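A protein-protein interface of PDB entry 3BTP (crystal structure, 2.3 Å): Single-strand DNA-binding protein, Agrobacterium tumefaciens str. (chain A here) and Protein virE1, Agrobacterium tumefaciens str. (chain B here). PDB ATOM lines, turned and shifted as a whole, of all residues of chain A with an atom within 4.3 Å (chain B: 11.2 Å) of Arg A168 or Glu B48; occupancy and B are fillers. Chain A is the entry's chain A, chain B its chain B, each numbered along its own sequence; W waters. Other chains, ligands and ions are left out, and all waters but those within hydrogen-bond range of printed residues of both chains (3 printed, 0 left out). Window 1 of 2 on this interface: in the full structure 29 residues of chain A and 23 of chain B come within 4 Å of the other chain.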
ATOM      1  N   TYR A 160     -15.576  -7.754  19.093  1.00  0.00           N
ATOM      2  CA  TYR A 160     -15.993  -7.142  20.372  1.00  0.00           C
ATOM      3  C   TYR A 160     -14.836  -6.428  20.991  1.00  0.00           C
ATOM      4  O   TYR A 160     -13.747  -6.990  21.074  1.00  0.00           O
ATOM      5  CB  TYR A 160     -16.412  -8.207  21.397  1.00  0.00           C
ATOM      6  CG  TYR A 160     -17.774  -8.828  21.174  1.00  0.00           C
ATOM      7  CD1 TYR A 160     -18.854  -8.456  21.975  1.00  0.00           C
ATOM      8  CD2 TYR A 160     -17.992  -9.768  20.152  1.00  0.00           C
ATOM      9  CE1 TYR A 160     -20.087  -9.021  21.801  1.00  0.00           C
ATOM     10  CE2 TYR A 160     -19.247 -10.316  19.936  1.00  0.00           C
ATOM     11  CZ  TYR A 160     -20.297  -9.942  20.778  1.00  0.00           C
ATOM     12  OH  TYR A 160     -21.555 -10.509  20.654  1.00  0.00           O
ATOM     13  N   LEU A 164     -17.280  -5.360  26.503  1.00  0.00           N
ATOM     14  CA  LEU A 164     -18.283  -6.243  25.905  1.00  0.00           C
ATOM     15  C   LEU A 164     -17.827  -7.664  25.662  1.00  0.00           C
ATOM     16  O   LEU A 164     -18.578  -8.544  25.862  1.00  0.00           O
ATOM     17  CB  LEU A 164     -18.817  -5.616  24.596  1.00  0.00           C
ATOM     18  CG  LEU A 164     -19.457  -4.211  24.745  1.00  0.00           C
ATOM     19  CD1 LEU A 164     -19.933  -3.730  23.412  1.00  0.00           C
ATOM     20  CD2 LEU A 164     -20.574  -4.075  25.749  1.00  0.00           C
ATOM     21  N   ALA A 165     -16.608  -7.887  25.176  1.00  0.00           N
ATOM     22  CA  ALA A 165     -16.084  -9.226  25.089  1.00  0.00           C
ATOM     23  C   ALA A 165     -16.109  -9.937  26.420  1.00  0.00           C
ATOM     24  O   ALA A 165     -16.416 -11.128  26.483  1.00  0.00           O
ATOM     25  CB  ALA A 165     -14.564  -9.246  24.421  1.00  0.00           C
ATOM     26  N   PHE A 166     -15.732  -9.226  27.491  1.00  0.00           N
ATOM     27  CA  PHE A 166     -15.753  -9.783  28.841  1.00  0.00           C
ATOM     28  C   PHE A 166     -17.169 -10.230  29.258  1.00  0.00           C
ATOM     29  O   PHE A 166     -17.378 -11.372  29.687  1.00  0.00           O
ATOM     30  CB  PHE A 166     -15.228  -8.746  29.831  1.00  0.00           C
ATOM     31  CG  PHE A 166     -15.057  -9.307  31.262  1.00  0.00           C
ATOM     32  CD1 PHE A 166     -13.912  -9.990  31.646  1.00  0.00           C
ATOM     33  CD2 PHE A 166     -16.016  -9.123  32.200  1.00  0.00           C
ATOM     34  CE1 PHE A 166     -13.801 -10.515  32.946  1.00  0.00           C
ATOM     35  CE2 PHE A 166     -15.888  -9.638  33.475  1.00  0.00           C
ATOM     36  CZ  PHE A 166     -14.787 -10.337  33.827  1.00  0.00           C
ATOM     37  N   GLU A 167     -18.146  -9.326  29.170  1.00  0.00           N
ATOM     38  CA  GLU A 167     -19.527  -9.670  29.583  1.00  0.00           C
ATOM     39  C   GLU A 167     -20.168 -10.722  28.679  1.00  0.00           C
ATOM     40  O   GLU A 167     -21.100 -11.420  29.102  1.00  0.00           O
ATOM     41  CB  GLU A 167     -20.420  -8.405  29.731  1.00  0.00           C
ATOM     42  CG  GLU A 167     -20.020  -7.628  31.041  1.00  0.00           C
ATOM     43  CD  GLU A 167     -20.200  -8.505  32.335  1.00  0.00           C
ATOM     44  OE1 GLU A 167     -20.857  -9.583  32.261  1.00  0.00           O
ATOM     45  OE2 GLU A 167     -19.744  -8.136  33.427  1.00  0.00           O
ATOM     46  N   ARG A 168     -19.693 -10.843  27.456  1.00  0.00           N
ATOM     47  CA  ARG A 168     -20.197 -11.878  26.540  1.00  0.00           C
ATOM     48  C   ARG A 168     -19.794 -13.302  26.973  1.00  0.00           C
ATOM     49  O   ARG A 168     -20.393 -14.288  26.529  1.00  0.00           O
ATOM     50  CB  ARG A 168     -19.767 -11.560  25.084  1.00  0.00           C
ATOM     51  CG  ARG A 168     -19.810 -12.705  24.041  1.00  0.00           C
ATOM     52  CD  ARG A 168     -21.150 -12.669  23.384  1.00  0.00           C
ATOM     53  NE  ARG A 168     -21.616 -13.784  22.513  1.00  0.00           N
ATOM     54  CZ  ARG A 168     -22.162 -14.904  22.958  1.00  0.00           C
ATOM     55  NH1 ARG A 168     -22.172 -15.199  24.257  1.00  0.00           N
ATOM     56  NH2 ARG A 168     -22.674 -15.749  22.095  1.00  0.00           N
ATOM     57  N   ILE A 169     -18.804 -13.434  27.854  1.00  0.00           N
ATOM     58  CA  ILE A 169     -18.563 -14.748  28.461  1.00  0.00           C
ATOM     59  C   ILE A 169     -19.832 -15.159  29.211  1.00  0.00           C
ATOM     60  O   ILE A 169     -20.414 -14.371  30.001  1.00  0.00           O
ATOM     61  CB  ILE A 169     -17.302 -14.836  29.351  1.00  0.00           C
ATOM     62  CG1 ILE A 169     -15.988 -14.432  28.575  1.00  0.00           C
ATOM     63  CG2 ILE A 169     -17.206 -16.290  29.954  1.00  0.00           C
ATOM     64  CD1 ILE A 169     -14.805 -13.690  29.454  1.00  0.00           C
ATOM     65  N   ASP A 170     -20.350 -16.340  28.929  1.00  0.00           N
ATOM     66  CA  ASP A 170     -21.630 -16.689  29.564  1.00  0.00           C
ATOM     67  C   ASP A 170     -21.393 -17.602  30.775  1.00  0.00           C
ATOM     68  O   ASP A 170     -20.399 -18.306  30.833  1.00  0.00           O
ATOM     69  CB  ASP A 170     -22.618 -17.334  28.591  1.00  0.00           C
ATOM     70  CG  ASP A 170     -22.126 -18.647  28.103  1.00  0.00           C
ATOM     71  OD1 ASP A 170     -20.919 -18.703  27.788  1.00  0.00           O
ATOM     72  OD2 ASP A 170     -22.923 -19.640  28.072  1.00  0.00           O
ATOM     73  N   TYR A 319     -23.270 -12.033   9.064  1.00  0.00           N
ATOM     74  CA  TYR A 319     -24.000 -12.324  10.310  1.00  0.00           C
ATOM     75  C   TYR A 319     -25.342 -11.503  10.432  1.00  0.00           C
ATOM     76  O   TYR A 319     -26.426 -12.030  10.754  1.00  0.00           O
ATOM     77  CB  TYR A 319     -23.152 -12.091  11.562  1.00  0.00           C
ATOM     78  CG  TYR A 319     -23.937 -12.547  12.759  1.00  0.00           C
ATOM     79  CD1 TYR A 319     -24.246 -13.888  12.929  1.00  0.00           C
ATOM     80  CD2 TYR A 319     -24.459 -11.631  13.667  1.00  0.00           C
ATOM     81  CE1 TYR A 319     -24.987 -14.329  14.011  1.00  0.00           C
ATOM     82  CE2 TYR A 319     -25.203 -12.042  14.768  1.00  0.00           C
ATOM     83  CZ  TYR A 319     -25.491 -13.394  14.915  1.00  0.00           C
ATOM     84  OH  TYR A 319     -26.222 -13.836  16.001  1.00  0.00           O
ATOM     85  N   TYR A 373     -30.026 -19.551   9.412  1.00  0.00           N
ATOM     86  CA  TYR A 373     -29.273 -19.074  10.574  1.00  0.00           C
ATOM     87  C   TYR A 373     -28.364 -20.174  11.185  1.00  0.00           C
ATOM     88  O   TYR A 373     -27.155 -20.011  11.360  1.00  0.00           O
ATOM     89  CB  TYR A 373     -30.254 -18.489  11.641  1.00  0.00           C
ATOM     90  CG  TYR A 373     -29.563 -17.870  12.816  1.00  0.00           C
ATOM     91  CD1 TYR A 373     -29.098 -16.532  12.780  1.00  0.00           C
ATOM     92  CD2 TYR A 373     -29.317 -18.608  13.937  1.00  0.00           C
ATOM     93  CE1 TYR A 373     -28.429 -15.942  13.878  1.00  0.00           C
ATOM     94  CE2 TYR A 373     -28.618 -18.060  15.028  1.00  0.00           C
ATOM     95  CZ  TYR A 373     -28.173 -16.748  14.990  1.00  0.00           C
ATOM     96  OH  TYR A 373     -27.536 -16.287  16.124  1.00  0.00           O
ATOM     97  N   HIS B  32     -24.946  -3.295  35.357  1.00  0.00           N
ATOM     98  CA  HIS B  32     -23.723  -2.903  34.645  1.00  0.00           C
ATOM     99  C   HIS B  32     -23.088  -3.985  33.718  1.00  0.00           C
ATOM    100  O   HIS B  32     -22.248  -3.670  32.884  1.00  0.00           O
ATOM    101  CB  HIS B  32     -22.708  -2.351  35.651  1.00  0.00           C
ATOM    102  CG  HIS B  32     -22.068  -3.421  36.479  1.00  0.00           C
ATOM    103  ND1 HIS B  32     -22.661  -3.934  37.615  1.00  0.00           N
ATOM    104  CD2 HIS B  32     -20.911  -4.110  36.308  1.00  0.00           C
ATOM    105  CE1 HIS B  32     -21.888  -4.883  38.118  1.00  0.00           C
ATOM    106  NE2 HIS B  32     -20.827  -5.019  37.338  1.00  0.00           N
ATOM    107  N   GLN B  33     -23.504  -5.240  33.888  1.00  0.00           N
ATOM    108  CA  GLN B  33     -23.106  -6.381  33.042  1.00  0.00           C
ATOM    109  C   GLN B  33     -23.774  -6.416  31.619  1.00  0.00           C
ATOM    110  O   GLN B  33     -23.315  -7.166  30.692  1.00  0.00           O
ATOM    111  CB  GLN B  33     -23.443  -7.705  33.776  1.00  0.00           C
ATOM    112  CG  GLN B  33     -22.733  -7.853  35.112  1.00  0.00           C
ATOM    113  CD  GLN B  33     -23.384  -7.082  36.301  1.00  0.00           C
ATOM    114  OE1 GLN B  33     -24.381  -6.333  36.137  1.00  0.00           O
ATOM    115  NE2 GLN B  33     -22.822  -7.285  37.508  1.00  0.00           N
ATOM    116  N   SER B  34     -24.891  -5.685  31.482  1.00  0.00           N
ATOM    117  CA  SER B  34     -25.682  -5.724  30.243  1.00  0.00           C
ATOM    118  C   SER B  34     -25.994  -4.322  29.653  1.00  0.00           C
ATOM    119  O   SER B  34     -26.277  -4.207  28.488  1.00  0.00           O
ATOM    120  CB  SER B  34     -26.957  -6.535  30.435  1.00  0.00           C
ATOM    121  OG  SER B  34     -27.815  -5.834  31.296  1.00  0.00           O
ATOM    122  N   ASN B  35     -25.845  -3.261  30.443  1.00  0.00           N
ATOM    123  CA  ASN B  35     -26.210  -1.922  29.994  1.00  0.00           C
ATOM    124  C   ASN B  35     -25.275  -1.253  28.982  1.00  0.00           C
ATOM    125  O   ASN B  35     -25.611  -0.205  28.437  1.00  0.00           O
ATOM    126  CB  ASN B  35     -26.555  -1.047  31.192  1.00  0.00           C
ATOM    127  CG  ASN B  35     -25.283  -0.597  32.030  1.00  0.00           C
ATOM    128  OD1 ASN B  35     -24.114  -0.841  31.666  1.00  0.00           O
ATOM    129  ND2 ASN B  35     -25.551   0.090  33.148  1.00  0.00           N
ATOM    130  N   GLY B  36     -24.134  -1.877  28.651  1.00  0.00           N
ATOM    131  CA  GLY B  36     -23.277  -1.379  27.561  1.00  0.00           C
ATOM    132  C   GLY B  36     -23.725  -1.970  26.238  1.00  0.00           C
ATOM    133  O   GLY B  36     -23.192  -1.625  25.195  1.00  0.00           O
ATOM    134  N   PHE B  37     -24.664  -2.922  26.311  1.00  0.00           N
ATOM    135  CA  PHE B  37     -25.198  -3.594  25.122  1.00  0.00           C
ATOM    136  C   PHE B  37     -26.524  -2.963  24.653  1.00  0.00           C
ATOM    137  O   PHE B  37     -27.289  -2.426  25.414  1.00  0.00           O
ATOM    138  CB  PHE B  37     -25.468  -5.058  25.370  1.00  0.00           C
ATOM    139  CG  PHE B  37     -24.189  -5.940  25.606  1.00  0.00           C
ATOM    140  CD1 PHE B  37     -23.787  -6.255  26.905  1.00  0.00           C
ATOM    141  CD2 PHE B  37     -23.456  -6.478  24.511  1.00  0.00           C
ATOM    142  CE1 PHE B  37     -22.670  -7.128  27.133  1.00  0.00           C
ATOM    143  CE2 PHE B  37     -22.296  -7.337  24.719  1.00  0.00           C
ATOM    144  CZ  PHE B  37     -21.939  -7.687  26.036  1.00  0.00           C
ATOM    145  N   THR B  38     -26.722  -3.007  23.363  1.00  0.00           N
ATOM    146  CA  THR B  38     -27.964  -2.600  22.707  1.00  0.00           C
ATOM    147  C   THR B  38     -28.992  -3.704  23.001  1.00  0.00           C
ATOM    148  O   THR B  38     -28.627  -4.836  23.262  1.00  0.00           O
ATOM    149  CB  THR B  38     -27.553  -2.468  21.262  1.00  0.00           C
ATOM    150  OG1 THR B  38     -27.325  -1.122  20.869  1.00  0.00           O
ATOM    151  CG2 THR B  38     -28.108  -3.363  20.356  1.00  0.00           C
ATOM    152  N   SER B  39     -30.270  -3.386  22.918  1.00  0.00           N
ATOM    153  CA  SER B  39     -31.310  -4.374  23.093  1.00  0.00           C
ATOM    154  C   SER B  39     -31.159  -5.463  22.038  1.00  0.00           C
ATOM    155  O   SER B  39     -31.287  -6.653  22.363  1.00  0.00           O
ATOM    156  CB  SER B  39     -32.695  -3.689  22.965  1.00  0.00           C
ATOM    157  OG  SER B  39     -32.958  -2.970  24.174  1.00  0.00           O
ATOM    158  N   LEU B  40     -30.930  -5.057  20.775  1.00  0.00           N
ATOM    159  CA  LEU B  40     -30.645  -5.992  19.711  1.00  0.00           C
ATOM    160  C   LEU B  40     -29.371  -6.851  19.945  1.00  0.00           C
ATOM    161  O   LEU B  40     -29.419  -8.050  19.742  1.00  0.00           O
ATOM    162  CB  LEU B  40     -30.592  -5.298  18.352  1.00  0.00           C
ATOM    163  CG  LEU B  40     -30.451  -6.240  17.101  1.00  0.00           C
ATOM    164  CD1 LEU B  40     -31.672  -7.151  16.909  1.00  0.00           C
ATOM    165  CD2 LEU B  40     -30.177  -5.455  15.743  1.00  0.00           C
ATOM    166  N   ASP B  41     -28.251  -6.267  20.382  1.00  0.00           N
ATOM    167  CA  ASP B  41     -27.049  -7.086  20.676  1.00  0.00           C
ATOM    168  C   ASP B  41     -27.368  -8.155  21.699  1.00  0.00           C
ATOM    169  O   ASP B  41     -26.880  -9.220  21.599  1.00  0.00           O
ATOM    170  CB  ASP B  41     -25.892  -6.309  21.290  1.00  0.00           C
ATOM    171  CG  ASP B  41     -25.425  -5.151  20.496  1.00  0.00           C
ATOM    172  OD1 ASP B  41     -25.466  -5.135  19.230  1.00  0.00           O
ATOM    173  OD2 ASP B  41     -24.927  -4.247  21.198  1.00  0.00           O
ATOM    174  N   LEU B  42     -28.217  -7.867  22.675  1.00  0.00           N
ATOM    175  CA  LEU B  42     -28.592  -8.853  23.721  1.00  0.00           C
ATOM    176  C   LEU B  42     -29.514  -9.994  23.256  1.00  0.00           C
ATOM    177  O   LEU B  42     -29.390 -11.148  23.710  1.00  0.00           O
ATOM    178  CB  LEU B  42     -29.236  -8.134  24.942  1.00  0.00           C
ATOM    179  CG  LEU B  42     -28.403  -7.113  25.754  1.00  0.00           C
ATOM    180  CD1 LEU B  42     -29.237  -6.436  26.897  1.00  0.00           C
ATOM    181  CD2 LEU B  42     -27.183  -7.867  26.342  1.00  0.00           C
ATOM    182  N   GLU B  43     -30.437  -9.685  22.373  1.00  0.00           N
ATOM    183  CA  GLU B  43     -31.207 -10.735  21.668  1.00  0.00           C
ATOM    184  C   GLU B  43     -30.365 -11.579  20.790  1.00  0.00           C
ATOM    185  O   GLU B  43     -30.633 -12.748  20.686  1.00  0.00           O
ATOM    186  CB  GLU B  43     -32.334 -10.169  20.770  1.00  0.00           C
ATOM    187  CG  GLU B  43     -33.344  -9.355  21.516  1.00  0.00           C
ATOM    188  CD  GLU B  43     -34.186  -8.483  20.577  1.00  0.00           C
ATOM    189  OE1 GLU B  43     -34.272  -8.792  19.355  1.00  0.00           O
ATOM    190  OE2 GLU B  43     -34.751  -7.472  21.043  1.00  0.00           O
ATOM    191  N   MET B  44     -29.380 -10.977  20.100  1.00  0.00           N
ATOM    192  CA  MET B  44     -28.443 -11.747  19.284  1.00  0.00           C
ATOM    193  C   MET B  44     -27.695 -12.718  20.187  1.00  0.00           C
ATOM    194  O   MET B  44     -27.680 -13.926  19.961  1.00  0.00           O
ATOM    195  CB  MET B  44     -27.452 -10.815  18.550  1.00  0.00           C
ATOM    196  CG  MET B  44     -28.041 -10.144  17.312  1.00  0.00           C
ATOM    197  SD  MET B  44     -27.018  -8.891  16.502  1.00  0.00           S
ATOM    198  CE  MET B  44     -27.962  -8.854  15.023  1.00  0.00           C
ATOM    199  N   ILE B  45     -27.063 -12.198  21.222  1.00  0.00           N
ATOM    200  CA  ILE B  45     -26.344 -13.059  22.191  1.00  0.00           C
ATOM    201  C   ILE B  45     -27.187 -14.144  22.847  1.00  0.00           C
ATOM    202  O   ILE B  45     -26.764 -15.318  22.889  1.00  0.00           O
ATOM    203  CB  ILE B  45     -25.676 -12.181  23.263  1.00  0.00           C
ATOM    204  CG1 ILE B  45     -24.599 -11.310  22.601  1.00  0.00           C
ATOM    205  CG2 ILE B  45     -25.213 -13.005  24.457  1.00  0.00           C
ATOM    206  CD1 ILE B  45     -24.074 -10.153  23.508  1.00  0.00           C
ATOM    207  N   GLU B  46     -28.367 -13.773  23.360  1.00  0.00           N
ATOM    208  CA  GLU B  46     -29.334 -14.757  23.914  1.00  0.00           C
ATOM    209  C   GLU B  46     -29.550 -15.943  22.950  1.00  0.00           C
ATOM    210  O   GLU B  46     -29.546 -17.114  23.387  1.00  0.00           O
ATOM    211  CB  GLU B  46     -30.697 -14.115  24.331  1.00  0.00           C
ATOM    212  CG  GLU B  46     -31.603 -15.067  25.253  1.00  0.00           C
ATOM    213  CD  GLU B  46     -32.452 -16.103  24.424  1.00  0.00           C
ATOM    214  OE1 GLU B  46     -32.686 -15.821  23.221  1.00  0.00           O
ATOM    215  OE2 GLU B  46     -32.919 -17.183  24.959  1.00  0.00           O
ATOM    216  N   LEU B  47     -29.747 -15.668  21.665  1.00  0.00           N
ATOM    217  CA  LEU B  47     -30.049 -16.781  20.694  1.00  0.00           C
ATOM    218  C   LEU B  47     -28.792 -17.633  20.408  1.00  0.00           C
ATOM    219  O   LEU B  47     -28.863 -18.853  20.335  1.00  0.00           O
ATOM    220  CB  LEU B  47     -30.622 -16.198  19.359  1.00  0.00           C
ATOM    221  CG  LEU B  47     -30.983 -17.250  18.265  1.00  0.00           C
ATOM    222  CD1 LEU B  47     -31.975 -18.296  18.844  1.00  0.00           C
ATOM    223  CD2 LEU B  47     -31.554 -16.637  17.049  1.00  0.00           C
ATOM    224  N   GLU B  48     -27.651 -16.968  20.205  1.00  0.00           N
ATOM    225  CA  GLU B  48     -26.363 -17.621  20.072  1.00  0.00           C
ATOM    226  C   GLU B  48     -26.123 -18.542  21.245  1.00  0.00           C
ATOM    227  O   GLU B  48     -25.838 -19.714  21.009  1.00  0.00           O
ATOM    228  CB  GLU B  48     -25.191 -16.645  19.908  1.00  0.00           C
ATOM    229  CG  GLU B  48     -25.257 -15.703  18.734  1.00  0.00           C
ATOM    230  CD  GLU B  48     -24.385 -14.406  18.917  1.00  0.00           C
ATOM    231  OE1 GLU B  48     -23.506 -14.426  19.820  1.00  0.00           O
ATOM    232  OE2 GLU B  48     -24.590 -13.392  18.150  1.00  0.00           O
ATOM    233  N   ASN B  49     -26.278 -18.053  22.477  1.00  0.00           N
ATOM    234  CA  ASN B  49     -26.118 -18.903  23.689  1.00  0.00           C
ATOM    235  C   ASN B  49     -27.126 -20.053  23.743  1.00  0.00           C
ATOM    236  O   ASN B  49     -26.804 -21.148  24.125  1.00  0.00           O
ATOM    237  CB  ASN B  49     -26.289 -18.071  25.000  1.00  0.00           C
ATOM    238  CG  ASN B  49     -25.123 -17.138  25.268  1.00  0.00           C
ATOM    239  OD1 ASN B  49     -24.042 -17.199  24.616  1.00  0.00           O
ATOM    240  ND2 ASN B  49     -25.335 -16.236  26.219  1.00  0.00           N
ATOM    241  N   PHE B  50     -28.357 -19.778  23.366  1.00  0.00           N
ATOM    242  CA  PHE B  50     -29.437 -20.785  23.368  1.00  0.00           C
ATOM    243  C   PHE B  50     -29.052 -21.950  22.445  1.00  0.00           C
ATOM    244  O   PHE B  50     -29.103 -23.093  22.836  1.00  0.00           O
ATOM    245  CB  PHE B  50     -30.817 -20.190  22.884  1.00  0.00           C
ATOM    246  CG  PHE B  50     -31.820 -21.266  22.672  1.00  0.00           C
ATOM    247  CD1 PHE B  50     -32.424 -21.905  23.801  1.00  0.00           C
ATOM    248  CD2 PHE B  50     -32.071 -21.764  21.395  1.00  0.00           C
ATOM    249  CE1 PHE B  50     -33.317 -22.996  23.612  1.00  0.00           C
ATOM    250  CE2 PHE B  50     -32.927 -22.796  21.202  1.00  0.00           C
ATOM    251  CZ  PHE B  50     -33.546 -23.457  22.312  1.00  0.00           C
ATOM    252  N   VAL B  51     -28.595 -21.584  21.255  1.00  0.00           N
ATOM    253  CA  VAL B  51     -28.371 -22.446  20.152  1.00  0.00           C
ATOM    254  C   VAL B  51     -27.041 -23.223  20.321  1.00  0.00           C
ATOM    255  O   VAL B  51     -26.987 -24.400  19.954  1.00  0.00           O
ATOM    256  CB  VAL B  51     -28.588 -21.548  18.849  1.00  0.00           C
ATOM    257  CG1 VAL B  51     -27.401 -21.442  17.850  1.00  0.00           C
ATOM    258  CG2 VAL B  51     -30.050 -21.628  18.275  1.00  0.00           C
ATOM    259  N   LEU B  52     -26.025 -22.605  20.971  1.00  0.00           N
ATOM    260  CA  LEU B  52     -24.750 -23.252  21.351  1.00  0.00           C
ATOM    261  C   LEU B  52     -24.902 -24.351  22.436  1.00  0.00           C
ATOM    262  O   LEU B  52     -24.153 -25.322  22.440  1.00  0.00           O
ATOM    263  CB  LEU B  52     -23.749 -22.183  21.868  1.00  0.00           C
ATOM    264  CG  LEU B  52     -23.104 -21.290  20.791  1.00  0.00           C
ATOM    265  CD1 LEU B  52     -22.318 -20.098  21.452  1.00  0.00           C
ATOM    266  CD2 LEU B  52     -22.197 -22.158  19.885  1.00  0.00           C
ATOM    267  N   HIS B  53     -25.885 -24.199  23.333  1.00  0.00           N
ATOM    268  CA  HIS B  53     -26.048 -25.081  24.491  1.00  0.00           C
ATOM    269  C   HIS B  53     -27.316 -25.943  24.444  1.00  0.00           C
ATOM    270  O   HIS B  53     -27.702 -26.537  25.445  1.00  0.00           O
ATOM    271  CB  HIS B  53     -26.002 -24.270  25.806  1.00  0.00           C
ATOM    272  CG  HIS B  53     -24.708 -23.526  25.988  1.00  0.00           C
ATOM    273  ND1 HIS B  53     -24.635 -22.143  26.010  1.00  0.00           N
ATOM    274  CD2 HIS B  53     -23.421 -23.971  26.009  1.00  0.00           C
ATOM    275  CE1 HIS B  53     -23.368 -21.770  26.057  1.00  0.00           C
ATOM    276  NE2 HIS B  53     -22.609 -22.859  26.056  1.00  0.00           N
ATOM    277  N   CYS B  54     -27.983 -25.984  23.307  1.00  0.00           N
ATOM    278  CA  CYS B  54     -29.255 -26.731  23.212  1.00  0.00           C
ATOM    279  C   CYS B  54     -28.989 -28.255  22.987  1.00  0.00           C
ATOM    280  O   CYS B  54     -28.373 -28.632  21.985  1.00  0.00           O
ATOM    281  CB  CYS B  54     -30.195 -26.161  22.103  1.00  0.00           C
ATOM    282  SG  CYS B  54     -31.920 -26.809  22.218  1.00  0.00           S
ATOM    283  N   PRO B  55     -29.477 -29.102  23.910  1.00  0.00           N
ATOM    284  CA  PRO B  55     -29.346 -30.563  23.805  1.00  0.00           C
ATOM    285  C   PRO B  55     -30.265 -31.106  22.683  1.00  0.00           C
ATOM    286  O   PRO B  55     -31.423 -30.666  22.518  1.00  0.00           O
ATOM    287  CB  PRO B  55     -29.845 -31.078  25.181  1.00  0.00           C
ATOM    288  CG  PRO B  55     -30.799 -30.039  25.646  1.00  0.00           C
ATOM    289  CD  PRO B  55     -30.253 -28.695  25.098  1.00  0.00           C
HETATM  290  O   HOH W   1     -21.520 -12.846  19.911  1.00  0.00           O
HETATM  291  O   HOH W   2     -23.927  -9.104  19.768  1.00  0.00           O
HETATM  292  O   HOH W   3     -23.156 -14.293  27.344  1.00  0.00           O
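The guanidinium group (NH2) of Arg A168 lies within salt-bridge range of the side-chain carboxylate (OE1) of Glu B48, at 2.8 Å. NH1 of Arg A168 lies within hydrogen-bond range of OD1 of Asn B49 (2.8 Å). The side-chain hydroxyl (OH) of Tyr A319 lies within hydrogen-bond range of the side-chain carboxylate (OE2) of Glu B48 (2.7 Å).
NE2 of His B32 sits close to NE2 of Gln B33, at 3.0 Å. A ring nitrogen (ND1) of His B53 lies within hydrogen-bond range of the backbone carbonyl oxygen of Asn B49. OH of Tyr A319 lies within hydrogen-bond range of OH of Tyr A373 (2.8 Å).
Ile B45 touches Tyr A160. O of Gly B36 touches CD2 of Leu A164, 3.6 Å away. CZ of Phe B37 touches O of Leu A164 (3.5 Å). CB of Glu A167 touches O of Gln B33 (3.3 Å). Phe B37 touches Glu A167 (CE1 to CB, 3.7 Å). Ile B45 touches Arg A168. CB of Asp A170 touches ND2 of Asn B49, 3.8 Å away. CE1 of His B53 touches OD2 of Asp A170, at 3.0 Å. CD2 of Leu B47 touches CE2 of Tyr A373 (3.8 Å). Tyr A373 touches Glu B48.
Arg A168 touches just these residues of chain B: Ile B45 (3.8 Å), Glu B48 (2.8 Å) and Asn B49 (2.8 Å). Glu B48 touches just these residues of chain A: Arg A168, Tyr A319 and Tyr A373. Of the printed residues of chain A, Asn B49 touches Arg A168 (2.8 Å) and Asp A170 (3.8 Å). Of the printed residues of chain B, Leu A164 touches Gly B36 (3.6 Å) and Phe B37 (3.5 Å). Of the printed residues of chain A, Gly B36 touches Leu A164 (3.6 Å). Printed residues of chain A within 4 Å of Phe B37: Leu A164 and Glu A167. Of the printed residues of chain B, Tyr A373 touches Leu B47 (3.8 Å) and Glu B48 (3.5 Å). Asp B41 touches none of the printed residues of chain A. The nearest printed residue of chain A that does not touch Glu B48 is Tyr A160 (4.5 Å).
Hydrophobic or aromatic side chains of chain B within 4 Å of the printed part of chain A: Phe B37, Ile B45, Leu B47 and His B53. Of the 10 printed residues of chain A, 7 touch a printed residue of chain B. Hydrophobic or aromatic side chains of chain A that line the printed part of chain B: Tyr A160, Leu A164, Tyr A319 and Tyr A373. Among the printed residues, 13 pairs touch across the chains. Among the printed residues, Asp or Glu carboxylates within 4 Å of a Lys or Arg side-chain nitrogen of the other chain: Arg A168 with Glu B48 (2.8 Å).
Water W1 lies within hydrogen-bond range of the side-chain hydroxyl (OH) of Tyr A160 (2.5 Å), the side-chain carboxylate (OE1) of Glu B48 (2.5 Å) and the guanidinium group (NE) of Arg A168 (2.8 Å). Water W3 bridges O of Arg A168 and ND2 of Asn B49. Water W2 bridges the side-chain hydroxyl (OH) of Tyr A160 and the backbone carbonyl oxygen (O) of Asp B41.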
